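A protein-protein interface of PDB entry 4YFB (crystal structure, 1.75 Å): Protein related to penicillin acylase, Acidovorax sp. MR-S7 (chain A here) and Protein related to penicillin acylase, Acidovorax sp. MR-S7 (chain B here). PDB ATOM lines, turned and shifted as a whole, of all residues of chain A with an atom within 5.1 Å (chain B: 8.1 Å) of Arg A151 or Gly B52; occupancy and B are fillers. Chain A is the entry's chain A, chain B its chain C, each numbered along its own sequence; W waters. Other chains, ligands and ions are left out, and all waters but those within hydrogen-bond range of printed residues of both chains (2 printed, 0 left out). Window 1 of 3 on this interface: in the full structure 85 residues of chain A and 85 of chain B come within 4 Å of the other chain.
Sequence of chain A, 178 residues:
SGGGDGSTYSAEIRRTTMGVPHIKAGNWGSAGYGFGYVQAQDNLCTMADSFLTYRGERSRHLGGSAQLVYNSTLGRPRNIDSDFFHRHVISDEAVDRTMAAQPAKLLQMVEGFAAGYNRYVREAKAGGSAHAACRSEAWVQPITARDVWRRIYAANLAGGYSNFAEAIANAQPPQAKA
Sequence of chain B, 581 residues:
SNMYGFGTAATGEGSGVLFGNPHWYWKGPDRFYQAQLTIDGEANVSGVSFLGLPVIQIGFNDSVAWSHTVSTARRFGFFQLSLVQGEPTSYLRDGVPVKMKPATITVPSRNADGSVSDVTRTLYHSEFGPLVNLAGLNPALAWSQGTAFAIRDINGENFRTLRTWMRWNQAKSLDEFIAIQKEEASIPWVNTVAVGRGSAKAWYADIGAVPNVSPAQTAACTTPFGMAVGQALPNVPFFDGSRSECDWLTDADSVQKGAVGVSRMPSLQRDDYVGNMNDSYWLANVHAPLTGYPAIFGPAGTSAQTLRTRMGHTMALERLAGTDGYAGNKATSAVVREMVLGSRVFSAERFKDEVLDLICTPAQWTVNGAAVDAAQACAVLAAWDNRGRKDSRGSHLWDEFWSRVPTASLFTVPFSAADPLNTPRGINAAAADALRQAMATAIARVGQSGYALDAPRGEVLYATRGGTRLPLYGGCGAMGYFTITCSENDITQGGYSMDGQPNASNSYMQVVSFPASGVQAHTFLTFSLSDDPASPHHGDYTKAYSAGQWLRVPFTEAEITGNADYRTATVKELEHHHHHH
Tyr B33 touches Gln A39 (CD2 to CG, 3.8 Å). Met A47 touches Gly B52. Tyr A54 touches Pro B29 (OH to CG, 3.4 Å). CE2 of Phe A113 touches O of Leu B53, at 3.9 Å. O of Gly B52 touches CG1 of Val A148, at 3.7 Å. CD2 of Leu B162 touches CH2 of Trp A149, 3.7 Å away. Phe B50 touches Arg A151 (CB to NH2, 3.6 Å). Arg A151 touches Gly B52. CD2 of Leu B53 touches CG1 of Ile A152 (3.5 Å). Leu B162 touches Ile A152 (CD2 to CD1, 3.999 Å).
Arg A151 touches six residues of chain B. Gly B52 touches five residues of chain A. Printed residues of chain A within 4 Å of Leu B51: Gln A39 and Arg A151. Printed residues of chain B within 4 Å of Tyr A54: Pro B29. Tyr A153 touches none of the printed residues of chain B. The nearest residue of chain B that does not touch Arg A151 is Arg B31 (5.8 Å). The nearest residue of chain A that does not touch Gly B52 is Ile A152 (4.6 Å).
Hydrophobic or aromatic side chains of chain A within 4 Å of the printed part of chain B: Met A47, Tyr A54, Phe A113, Val A148, Trp A149 and Ile A152. Printed residues of chain B that touch a printed residue of chain A: Pro B29, Asp B30, Tyr B33, Phe B50, Leu B51, Gly B52, Leu B53, Pro B54 and Leu B162. Hydrophobic or aromatic side chains of chain B within 4 Å of the printed part of chain A: Pro B29, Tyr B33, Phe B50, Leu B53, Pro B54 and Leu B162. Among the printed residues, 19 pairs touch across the chains.
OE1 of Gln A39 is in hydrogen-bond range of N of Gly B52, at 2.7 Å. The backbone carbonyl oxygen (O) of Leu B53 sits at hydrogen-bond distance from the side-chain amide nitrogen (NE2) of Gln A39. The backbone carbonyl oxygen (O) of Leu B51 is in hydrogen-bond range of the guanidinium group (NE) of Arg A151, at 2.7 Å. O of Pro B29 lies within hydrogen-bond range of NH2 of Arg A151, 2.9 Å away. The guanidinium group of Arg A151 lies within salt-bridge range of the side-chain carboxylate of Asp B30.
Water W1 lies within hydrogen-bond range of OH of Tyr A54 (2.8 Å) and OD1 of Asp B30 (2.9 Å). Water W2 lies within hydrogen-bond range of the side-chain carboxylate of Asp B30 (2.8 Å) and the guanidinium group of Arg A151 (2.9 Å).
The backbone carbonyl oxygen (O) of Arg B31 sits at hydrogen-bond distance from the backbone NH (N) of Leu B51 (3.0 Å). The indole nitrogen (NE1) of Trp B24 is in hydrogen-bond range of the backbone carbonyl oxygen (O) of Asp B30 (2.7 Å). The backbone carbonyl oxygen (O) of Pro B29 lies within hydrogen-bond range of the backbone NH (N) of Leu B51, 3.4 Å away. N of Tyr B33 is in hydrogen-bond range of O of Ser B49, at 2.9 Å. The side-chain amide oxygen (OE1) of Gln B57 lies within hydrogen-bond range of the backbone NH (N) of Phe B50, at 2.7 Å.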
ATOM      1  N   GLN A  39      19.730  -5.700  13.001  1.00  0.00           N
ATOM      2  CA  GLN A  39      18.979  -6.920  13.042  1.00  0.00           C
ATOM      3  C   GLN A  39      17.640  -6.661  12.307  1.00  0.00           C
ATOM      4  O   GLN A  39      17.231  -7.503  11.525  1.00  0.00           O
ATOM      5  CB  GLN A  39      18.657  -7.328  14.508  1.00  0.00           C
ATOM      6  CG  GLN A  39      19.864  -7.931  15.237  1.00  0.00           C
ATOM      7  CD  GLN A  39      19.485  -8.589  16.560  1.00  0.00           C
ATOM      8  OE1 GLN A  39      18.279  -8.945  16.777  1.00  0.00           O
ATOM      9  NE2 GLN A  39      20.475  -8.744  17.463  1.00  0.00           N
ATOM     10  N   MET A  47      11.286 -10.585  12.835  1.00  0.00           N
ATOM     11  CA  MET A  47      11.311  -9.995  14.184  1.00  0.00           C
ATOM     12  C   MET A  47       9.954  -9.387  14.518  1.00  0.00           C
ATOM     13  O   MET A  47       9.512  -9.452  15.659  1.00  0.00           O
ATOM     14  CB  MET A  47      12.335  -8.814  14.243  1.00  0.00           C
ATOM     15  CG  MET A  47      13.698  -9.431  14.149  1.00  0.00           C
ATOM     16  SD  MET A  47      15.074  -8.214  14.276  1.00  0.00           S
ATOM     17  CE  MET A  47      15.043  -7.884  16.087  1.00  0.00           C
ATOM     18  N   PHE A  51       7.635 -10.134  17.832  1.00  0.00           N
ATOM     19  CA  PHE A  51       7.185  -9.338  18.961  1.00  0.00           C
ATOM     20  C   PHE A  51       5.667  -9.447  19.203  1.00  0.00           C
ATOM     21  O   PHE A  51       5.245  -9.279  20.350  1.00  0.00           O
ATOM     22  CB  PHE A  51       7.629  -7.885  18.822  1.00  0.00           C
ATOM     23  CG  PHE A  51       9.104  -7.742  19.126  1.00  0.00           C
ATOM     24  CD1 PHE A  51       9.541  -7.837  20.453  1.00  0.00           C
ATOM     25  CD2 PHE A  51      10.014  -7.488  18.101  1.00  0.00           C
ATOM     26  CE1 PHE A  51      10.924  -7.789  20.776  1.00  0.00           C
ATOM     27  CE2 PHE A  51      11.379  -7.415  18.379  1.00  0.00           C
ATOM     28  CZ  PHE A  51      11.832  -7.519  19.721  1.00  0.00           C
ATOM     29  N   TYR A  54       5.667 -12.471  21.774  1.00  0.00           N
ATOM     30  CA  TYR A  54       6.086 -12.275  23.165  1.00  0.00           C
ATOM     31  C   TYR A  54       5.106 -11.336  23.907  1.00  0.00           C
ATOM     32  O   TYR A  54       4.965 -11.421  25.118  1.00  0.00           O
ATOM     33  CB  TYR A  54       7.514 -11.718  23.259  1.00  0.00           C
ATOM     34  CG  TYR A  54       8.490 -12.514  22.466  1.00  0.00           C
ATOM     35  CD1 TYR A  54       8.623 -13.903  22.674  1.00  0.00           C
ATOM     36  CD2 TYR A  54       9.173 -11.890  21.429  1.00  0.00           C
ATOM     37  CE1 TYR A  54       9.482 -14.671  21.859  1.00  0.00           C
ATOM     38  CE2 TYR A  54       9.998 -12.626  20.611  1.00  0.00           C
ATOM     39  CZ  TYR A  54      10.133 -13.963  20.816  1.00  0.00           C
ATOM     40  OH  TYR A  54      10.961 -14.608  19.985  1.00  0.00           O
ATOM     41  N   PHE A 113      18.414  -0.639  21.867  1.00  0.00           N
ATOM     42  CA  PHE A 113      18.029  -1.669  20.901  1.00  0.00           C
ATOM     43  C   PHE A 113      16.616  -1.459  20.417  1.00  0.00           C
ATOM     44  O   PHE A 113      16.366  -1.465  19.184  1.00  0.00           O
ATOM     45  CB  PHE A 113      18.192  -3.047  21.598  1.00  0.00           C
ATOM     46  CG  PHE A 113      18.075  -4.224  20.680  1.00  0.00           C
ATOM     47  CD1 PHE A 113      16.812  -4.721  20.328  1.00  0.00           C
ATOM     48  CD2 PHE A 113      19.215  -4.837  20.185  1.00  0.00           C
ATOM     49  CE1 PHE A 113      16.699  -5.852  19.499  1.00  0.00           C
ATOM     50  CE2 PHE A 113      19.090  -5.989  19.365  1.00  0.00           C
ATOM     51  CZ  PHE A 113      17.850  -6.463  19.030  1.00  0.00           C
ATOM     52  N   ASP A 147       9.198  -4.646  25.708  1.00  0.00           N
ATOM     53  CA  ASP A 147       8.987  -5.715  24.733  1.00  0.00           C
ATOM     54  C   ASP A 147      10.256  -6.510  24.469  1.00  0.00           C
ATOM     55  O   ASP A 147      10.205  -7.721  24.325  1.00  0.00           O
ATOM     56  CB  ASP A 147       8.487  -5.122  23.436  1.00  0.00           C
ATOM     57  CG  ASP A 147       7.086  -4.525  23.601  1.00  0.00           C
ATOM     58  OD1 ASP A 147       6.267  -4.983  24.469  1.00  0.00           O
ATOM     59  OD2 ASP A 147       6.790  -3.600  22.821  1.00  0.00           O
ATOM     60  N   VAL A 148      11.407  -5.844  24.428  1.00  0.00           N
ATOM     61  CA  VAL A 148      12.677  -6.567  24.273  1.00  0.00           C
ATOM     62  C   VAL A 148      12.982  -7.403  25.528  1.00  0.00           C
ATOM     63  O   VAL A 148      13.394  -8.571  25.409  1.00  0.00           O
ATOM     64  CB  VAL A 148      13.839  -5.597  23.976  1.00  0.00           C
ATOM     65  CG1 VAL A 148      15.171  -6.365  23.774  1.00  0.00           C
ATOM     66  CG2 VAL A 148      13.509  -4.840  22.669  1.00  0.00           C
ATOM     67  N   TRP A 149      12.715  -6.876  26.723  1.00  0.00           N
ATOM     68  CA  TRP A 149      12.800  -7.731  27.950  1.00  0.00           C
ATOM     69  C   TRP A 149      11.853  -8.886  27.939  1.00  0.00           C
ATOM     70  O   TRP A 149      12.232  -9.969  28.427  1.00  0.00           O
ATOM     71  CB  TRP A 149      12.602  -6.884  29.235  1.00  0.00           C
ATOM     72  CG  TRP A 149      13.806  -6.034  29.490  1.00  0.00           C
ATOM     73  CD1 TRP A 149      13.921  -4.652  29.323  1.00  0.00           C
ATOM     74  CD2 TRP A 149      15.152  -6.503  29.837  1.00  0.00           C
ATOM     75  NE1 TRP A 149      15.212  -4.226  29.618  1.00  0.00           N
ATOM     76  CE2 TRP A 149      15.994  -5.314  29.939  1.00  0.00           C
ATOM     77  CE3 TRP A 149      15.719  -7.794  30.096  1.00  0.00           C
ATOM     78  CZ2 TRP A 149      17.348  -5.397  30.274  1.00  0.00           C
ATOM     79  CZ3 TRP A 149      17.057  -7.846  30.492  1.00  0.00           C
ATOM     80  CH2 TRP A 149      17.872  -6.689  30.493  1.00  0.00           C
ATOM     81  N   ARG A 150      10.661  -8.720  27.317  1.00  0.00           N
ATOM     82  CA  ARG A 150       9.762  -9.862  27.118  1.00  0.00           C
ATOM     83  C   ARG A 150      10.444 -10.965  26.310  1.00  0.00           C
ATOM     84  O   ARG A 150      10.425 -12.130  26.690  1.00  0.00           O
ATOM     85  CB  ARG A 150       8.434  -9.520  26.467  1.00  0.00           C
ATOM     86  CG  ARG A 150       7.511  -8.685  27.318  1.00  0.00           C
ATOM     87  CD  ARG A 150       6.283  -8.317  26.438  1.00  0.00           C
ATOM     88  NE  ARG A 150       5.316  -7.860  27.415  1.00  0.00           N
ATOM     89  CZ  ARG A 150       5.261  -6.609  27.881  1.00  0.00           C
ATOM     90  NH1 ARG A 150       5.989  -5.635  27.348  1.00  0.00           N
ATOM     91  NH2 ARG A 150       4.400  -6.321  28.824  1.00  0.00           N
ATOM     92  N   ARG A 151      11.076 -10.583  25.204  1.00  0.00           N
ATOM     93  CA  ARG A 151      11.778 -11.525  24.341  1.00  0.00           C
ATOM     94  C   ARG A 151      12.978 -12.131  25.042  1.00  0.00           C
ATOM     95  O   ARG A 151      13.219 -13.339  24.924  1.00  0.00           O
ATOM     96  CB  ARG A 151      12.281 -10.747  23.093  1.00  0.00           C
ATOM     97  CG  ARG A 151      12.899 -11.690  22.010  1.00  0.00           C
ATOM     98  CD  ARG A 151      14.399 -11.987  22.216  1.00  0.00           C
ATOM     99  NE  ARG A 151      14.702 -12.963  21.161  1.00  0.00           N
ATOM    100  CZ  ARG A 151      14.365 -14.252  21.211  1.00  0.00           C
ATOM    101  NH1 ARG A 151      13.761 -14.746  22.312  1.00  0.00           N
ATOM    102  NH2 ARG A 151      14.598 -15.036  20.151  1.00  0.00           N
ATOM    103  N   ILE A 152      13.708 -11.337  25.817  1.00  0.00           N
ATOM    104  CA  ILE A 152      14.854 -11.862  26.568  1.00  0.00           C
ATOM    105  C   ILE A 152      14.391 -12.900  27.601  1.00  0.00           C
ATOM    106  O   ILE A 152      14.957 -14.030  27.707  1.00  0.00           O
ATOM    107  CB  ILE A 152      15.613 -10.690  27.236  1.00  0.00           C
ATOM    108  CG1 ILE A 152      16.315  -9.886  26.099  1.00  0.00           C
ATOM    109  CG2 ILE A 152      16.627 -11.194  28.289  1.00  0.00           C
ATOM    110  CD1 ILE A 152      16.638  -8.473  26.515  1.00  0.00           C
ATOM    111  N   TYR A 153      13.349 -12.540  28.376  1.00  0.00           N
ATOM    112  CA  TYR A 153      12.842 -13.496  29.378  1.00  0.00           C
ATOM    113  C   TYR A 153      12.328 -14.762  28.707  1.00  0.00           C
ATOM    114  O   TYR A 153      12.596 -15.889  29.166  1.00  0.00           O
ATOM    115  CB  TYR A 153      11.720 -12.838  30.176  1.00  0.00           C
ATOM    116  CG  TYR A 153      11.192 -13.670  31.340  1.00  0.00           C
ATOM    117  CD1 TYR A 153      12.000 -13.919  32.473  1.00  0.00           C
ATOM    118  CD2 TYR A 153       9.899 -14.191  31.301  1.00  0.00           C
ATOM    119  CE1 TYR A 153      11.471 -14.626  33.613  1.00  0.00           C
ATOM    120  CE2 TYR A 153       9.353 -14.900  32.419  1.00  0.00           C
ATOM    121  CZ  TYR A 153      10.154 -15.112  33.533  1.00  0.00           C
ATOM    122  OH  TYR A 153       9.652 -15.829  34.603  1.00  0.00           O
ATOM    123  N   ALA A 154      11.640 -14.596  27.577  1.00  0.00           N
ATOM    124  CA  ALA A 154      11.149 -15.784  26.827  1.00  0.00           C
ATOM    125  C   ALA A 154      12.227 -16.788  26.503  1.00  0.00           C
ATOM    126  O   ALA A 154      11.978 -18.010  26.616  1.00  0.00           O
ATOM    127  CB  ALA A 154      10.429 -15.377  25.520  1.00  0.00           C
ATOM    128  N   ALA A 155      13.407 -16.307  26.126  1.00  0.00           N
ATOM    129  CA  ALA A 155      14.524 -17.218  25.759  1.00  0.00           C
ATOM    130  C   ALA A 155      14.999 -18.069  26.964  1.00  0.00           C
ATOM    131  O   ALA A 155      15.495 -19.191  26.792  1.00  0.00           O
ATOM    132  CB  ALA A 155      15.687 -16.392  25.146  1.00  0.00           C
ATOM    133  N   TRP B  24      20.425 -25.735  14.994  1.00  0.00           N
ATOM    134  CA  TRP B  24      19.412 -24.819  15.497  1.00  0.00           C
ATOM    135  C   TRP B  24      18.549 -24.438  14.319  1.00  0.00           C
ATOM    136  O   TRP B  24      18.722 -24.959  13.189  1.00  0.00           O
ATOM    137  CB  TRP B  24      20.104 -23.581  16.135  1.00  0.00           C
ATOM    138  CG  TRP B  24      19.308 -22.794  17.137  1.00  0.00           C
ATOM    139  CD1 TRP B  24      18.993 -21.460  17.099  1.00  0.00           C
ATOM    140  CD2 TRP B  24      18.756 -23.284  18.385  1.00  0.00           C
ATOM    141  NE1 TRP B  24      18.302 -21.086  18.262  1.00  0.00           N
ATOM    142  CE2 TRP B  24      18.114 -22.133  19.036  1.00  0.00           C
ATOM    143  CE3 TRP B  24      18.741 -24.555  19.020  1.00  0.00           C
ATOM    144  CZ2 TRP B  24      17.471 -22.244  20.252  1.00  0.00           C
ATOM    145  CZ3 TRP B  24      18.076 -24.649  20.247  1.00  0.00           C
ATOM    146  CH2 TRP B  24      17.490 -23.497  20.858  1.00  0.00           C
ATOM    147  N   GLY B  28      12.851 -18.126  11.822  1.00  0.00           N
ATOM    148  CA  GLY B  28      12.118 -17.763  13.026  1.00  0.00           C
ATOM    149  C   GLY B  28      13.008 -16.947  13.965  1.00  0.00           C
ATOM    150  O   GLY B  28      14.249 -16.801  13.756  1.00  0.00           O
ATOM    151  N   PRO B  29      12.410 -16.492  15.071  1.00  0.00           N
ATOM    152  CA  PRO B  29      13.115 -15.472  15.859  1.00  0.00           C
ATOM    153  C   PRO B  29      14.182 -16.038  16.747  1.00  0.00           C
ATOM    154  O   PRO B  29      14.984 -15.263  17.293  1.00  0.00           O
ATOM    155  CB  PRO B  29      12.021 -14.872  16.710  1.00  0.00           C
ATOM    156  CG  PRO B  29      11.041 -16.017  16.887  1.00  0.00           C
ATOM    157  CD  PRO B  29      11.023 -16.669  15.492  1.00  0.00           C
ATOM    158  N   ASP B  30      14.266 -17.368  16.901  1.00  0.00           N
ATOM    159  CA  ASP B  30      15.353 -17.885  17.692  1.00  0.00           C
ATOM    160  C   ASP B  30      16.574 -18.179  16.792  1.00  0.00           C
ATOM    161  O   ASP B  30      17.597 -18.617  17.306  1.00  0.00           O
ATOM    162  CB  ASP B  30      14.906 -19.196  18.411  1.00  0.00           C
ATOM    163  CG  ASP B  30      13.973 -18.941  19.584  1.00  0.00           C
ATOM    164  OD1 ASP B  30      13.857 -17.795  20.062  1.00  0.00           O
ATOM    165  OD2 ASP B  30      13.471 -19.955  20.189  1.00  0.00           O
ATOM    166  N   ARG B  31      16.473 -17.924  15.483  1.00  0.00           N
ATOM    167  CA  ARG B  31      17.611 -18.160  14.616  1.00  0.00           C
ATOM    168  C   ARG B  31      18.738 -17.166  14.961  1.00  0.00           C
ATOM    169  O   ARG B  31      18.483 -16.047  15.490  1.00  0.00           O
ATOM    170  CB  ARG B  31      17.262 -18.131  13.135  1.00  0.00           C
ATOM    171  CG  ARG B  31      17.249 -16.763  12.514  1.00  0.00           C
ATOM    172  CD  ARG B  31      16.778 -16.932  11.048  1.00  0.00           C
ATOM    173  NE  ARG B  31      17.324 -15.819  10.220  1.00  0.00           N
ATOM    174  CZ  ARG B  31      17.312 -15.882   8.889  1.00  0.00           C
ATOM    175  NH1 ARG B  31      17.821 -14.924   8.127  1.00  0.00           N
ATOM    176  NH2 ARG B  31      16.781 -16.952   8.272  1.00  0.00           N
ATOM    177  N   TYR B  33      22.020 -14.557  14.396  1.00  0.00           N
ATOM    178  CA  TYR B  33      22.340 -13.361  13.681  1.00  0.00           C
ATOM    179  C   TYR B  33      23.788 -13.020  14.061  1.00  0.00           C
ATOM    180  O   TYR B  33      24.100 -12.869  15.213  1.00  0.00           O
ATOM    181  CB  TYR B  33      21.426 -12.215  14.054  1.00  0.00           C
ATOM    182  CG  TYR B  33      21.692 -10.948  13.212  1.00  0.00           C
ATOM    183  CD1 TYR B  33      21.093 -10.763  11.977  1.00  0.00           C
ATOM    184  CD2 TYR B  33      22.635  -9.977  13.666  1.00  0.00           C
ATOM    185  CE1 TYR B  33      21.360  -9.621  11.170  1.00  0.00           C
ATOM    186  CE2 TYR B  33      22.915  -8.858  12.894  1.00  0.00           C
ATOM    187  CZ  TYR B  33      22.297  -8.678  11.638  1.00  0.00           C
ATOM    188  OH  TYR B  33      22.490  -7.565  10.841  1.00  0.00           O
ATOM    189  N   SER B  49      23.762 -13.761  18.166  1.00  0.00           N
ATOM    190  CA  SER B  49      22.717 -13.659  19.154  1.00  0.00           C
ATOM    191  C   SER B  49      21.476 -14.270  18.446  1.00  0.00           C
ATOM    192  O   SER B  49      21.325 -14.133  17.197  1.00  0.00           O
ATOM    193  CB  SER B  49      22.347 -12.136  19.298  1.00  0.00           C
ATOM    194  OG  SER B  49      23.524 -11.481  19.809  1.00  0.00           O
ATOM    195  N   PHE B  50      20.514 -14.726  19.231  1.00  0.00           N
ATOM    196  CA  PHE B  50      19.162 -14.905  18.629  1.00  0.00           C
ATOM    197  C   PHE B  50      18.658 -13.555  18.142  1.00  0.00           C
ATOM    198  O   PHE B  50      18.997 -12.485  18.738  1.00  0.00           O
ATOM    199  CB  PHE B  50      18.142 -15.304  19.732  1.00  0.00           C
ATOM    200  CG  PHE B  50      18.392 -16.612  20.415  1.00  0.00           C
ATOM    201  CD1 PHE B  50      19.188 -17.611  19.836  1.00  0.00           C
ATOM    202  CD2 PHE B  50      17.667 -16.922  21.583  1.00  0.00           C
ATOM    203  CE1 PHE B  50      19.324 -18.842  20.462  1.00  0.00           C
ATOM    204  CE2 PHE B  50      17.813 -18.179  22.224  1.00  0.00           C
ATOM    205  CZ  PHE B  50      18.644 -19.125  21.671  1.00  0.00           C
ATOM    206  N   LEU B  51      17.866 -13.538  17.060  1.00  0.00           N
ATOM    207  CA  LEU B  51      17.171 -12.247  16.685  1.00  0.00           C
ATOM    208  C   LEU B  51      16.438 -11.717  17.936  1.00  0.00           C
ATOM    209  O   LEU B  51      15.720 -12.483  18.666  1.00  0.00           O
ATOM    210  CB  LEU B  51      16.187 -12.466  15.512  1.00  0.00           C
ATOM    211  CG  LEU B  51      16.948 -12.802  14.202  1.00  0.00           C
ATOM    212  CD1 LEU B  51      15.832 -13.110  13.156  1.00  0.00           C
ATOM    213  CD2 LEU B  51      17.652 -11.550  13.764  1.00  0.00           C
ATOM    214  N   GLY B  52      16.600 -10.429  18.205  1.00  0.00           N
ATOM    215  CA  GLY B  52      15.947  -9.747  19.329  1.00  0.00           C
ATOM    216  C   GLY B  52      16.771  -9.758  20.615  1.00  0.00           C
ATOM    217  O   GLY B  52      16.364  -9.106  21.558  1.00  0.00           O
ATOM    218  N   LEU B  53      17.900 -10.472  20.645  1.00  0.00           N
ATOM    219  CA  LEU B  53      18.826 -10.402  21.835  1.00  0.00           C
ATOM    220  C   LEU B  53      19.982  -9.439  21.532  1.00  0.00           C
ATOM    221  O   LEU B  53      20.495  -9.446  20.404  1.00  0.00           O
ATOM    222  CB  LEU B  53      19.390 -11.788  22.209  1.00  0.00           C
ATOM    223  CG  LEU B  53      18.325 -12.779  22.697  1.00  0.00           C
ATOM    224  CD1 LEU B  53      19.046 -14.036  23.092  1.00  0.00           C
ATOM    225  CD2 LEU B  53      17.522 -12.306  23.868  1.00  0.00           C
ATOM    226  N   PRO B  54      20.405  -8.640  22.540  1.00  0.00           N
ATOM    227  CA  PRO B  54      21.328  -7.522  22.351  1.00  0.00           C
ATOM    228  C   PRO B  54      22.801  -7.857  22.698  1.00  0.00           C
ATOM    229  O   PRO B  54      23.650  -6.995  22.399  1.00  0.00           O
ATOM    230  CB  PRO B  54      20.783  -6.423  23.299  1.00  0.00           C
ATOM    231  CG  PRO B  54      20.225  -7.221  24.423  1.00  0.00           C
ATOM    232  CD  PRO B  54      19.580  -8.462  23.763  1.00  0.00           C
ATOM    233  N   VAL B  55      23.080  -9.042  23.306  1.00  0.00           N
ATOM    234  CA  VAL B  55      24.493  -9.374  23.608  1.00  0.00           C
ATOM    235  C   VAL B  55      24.817 -10.673  22.880  1.00  0.00           C
ATOM    236  O   VAL B  55      23.882 -11.461  22.498  1.00  0.00           O
ATOM    237  CB  VAL B  55      24.804  -9.467  25.120  1.00  0.00           C
ATOM    238  CG1 VAL B  55      24.773  -8.071  25.802  1.00  0.00           C
ATOM    239  CG2 VAL B  55      23.973 -10.483  25.810  1.00  0.00           C
ATOM    240  N   GLN B  57      25.704 -14.422  22.283  1.00  0.00           N
ATOM    241  CA  GLN B  57      25.509 -15.654  23.063  1.00  0.00           C
ATOM    242  C   GLN B  57      26.536 -16.755  22.764  1.00  0.00           C
ATOM    243  O   GLN B  57      26.854 -17.602  23.656  1.00  0.00           O
ATOM    244  CB  GLN B  57      24.123 -16.255  22.719  1.00  0.00           C
ATOM    245  CG  GLN B  57      23.088 -15.401  23.410  1.00  0.00           C
ATOM    246  CD  GLN B  57      21.773 -15.697  22.769  1.00  0.00           C
ATOM    247  OE1 GLN B  57      21.481 -15.095  21.748  1.00  0.00           O
ATOM    248  NE2 GLN B  57      20.942 -16.598  23.397  1.00  0.00           N
ATOM    249  N   LEU B 162      21.198 -12.770  30.947  1.00  0.00           N
ATOM    250  CA  LEU B 162      21.741 -11.795  29.953  1.00  0.00           C
ATOM    251  C   LEU B 162      23.005 -11.139  30.481  1.00  0.00           C
ATOM    252  O   LEU B 162      23.977 -10.911  29.719  1.00  0.00           O
ATOM    253  CB  LEU B 162      20.672 -10.764  29.590  1.00  0.00           C
ATOM    254  CG  LEU B 162      21.020  -9.968  28.322  1.00  0.00           C
ATOM    255  CD1 LEU B 162      20.840 -10.874  27.153  1.00  0.00           C
ATOM    256  CD2 LEU B 162      20.192  -8.684  28.337  1.00  0.00           C
HETATM  257  O   HOH W   1      10.981 -17.366  20.104  1.00  0.00           O
HETATM  258  O   HOH W   2      13.106 -17.529  22.707  1.00  0.00           O
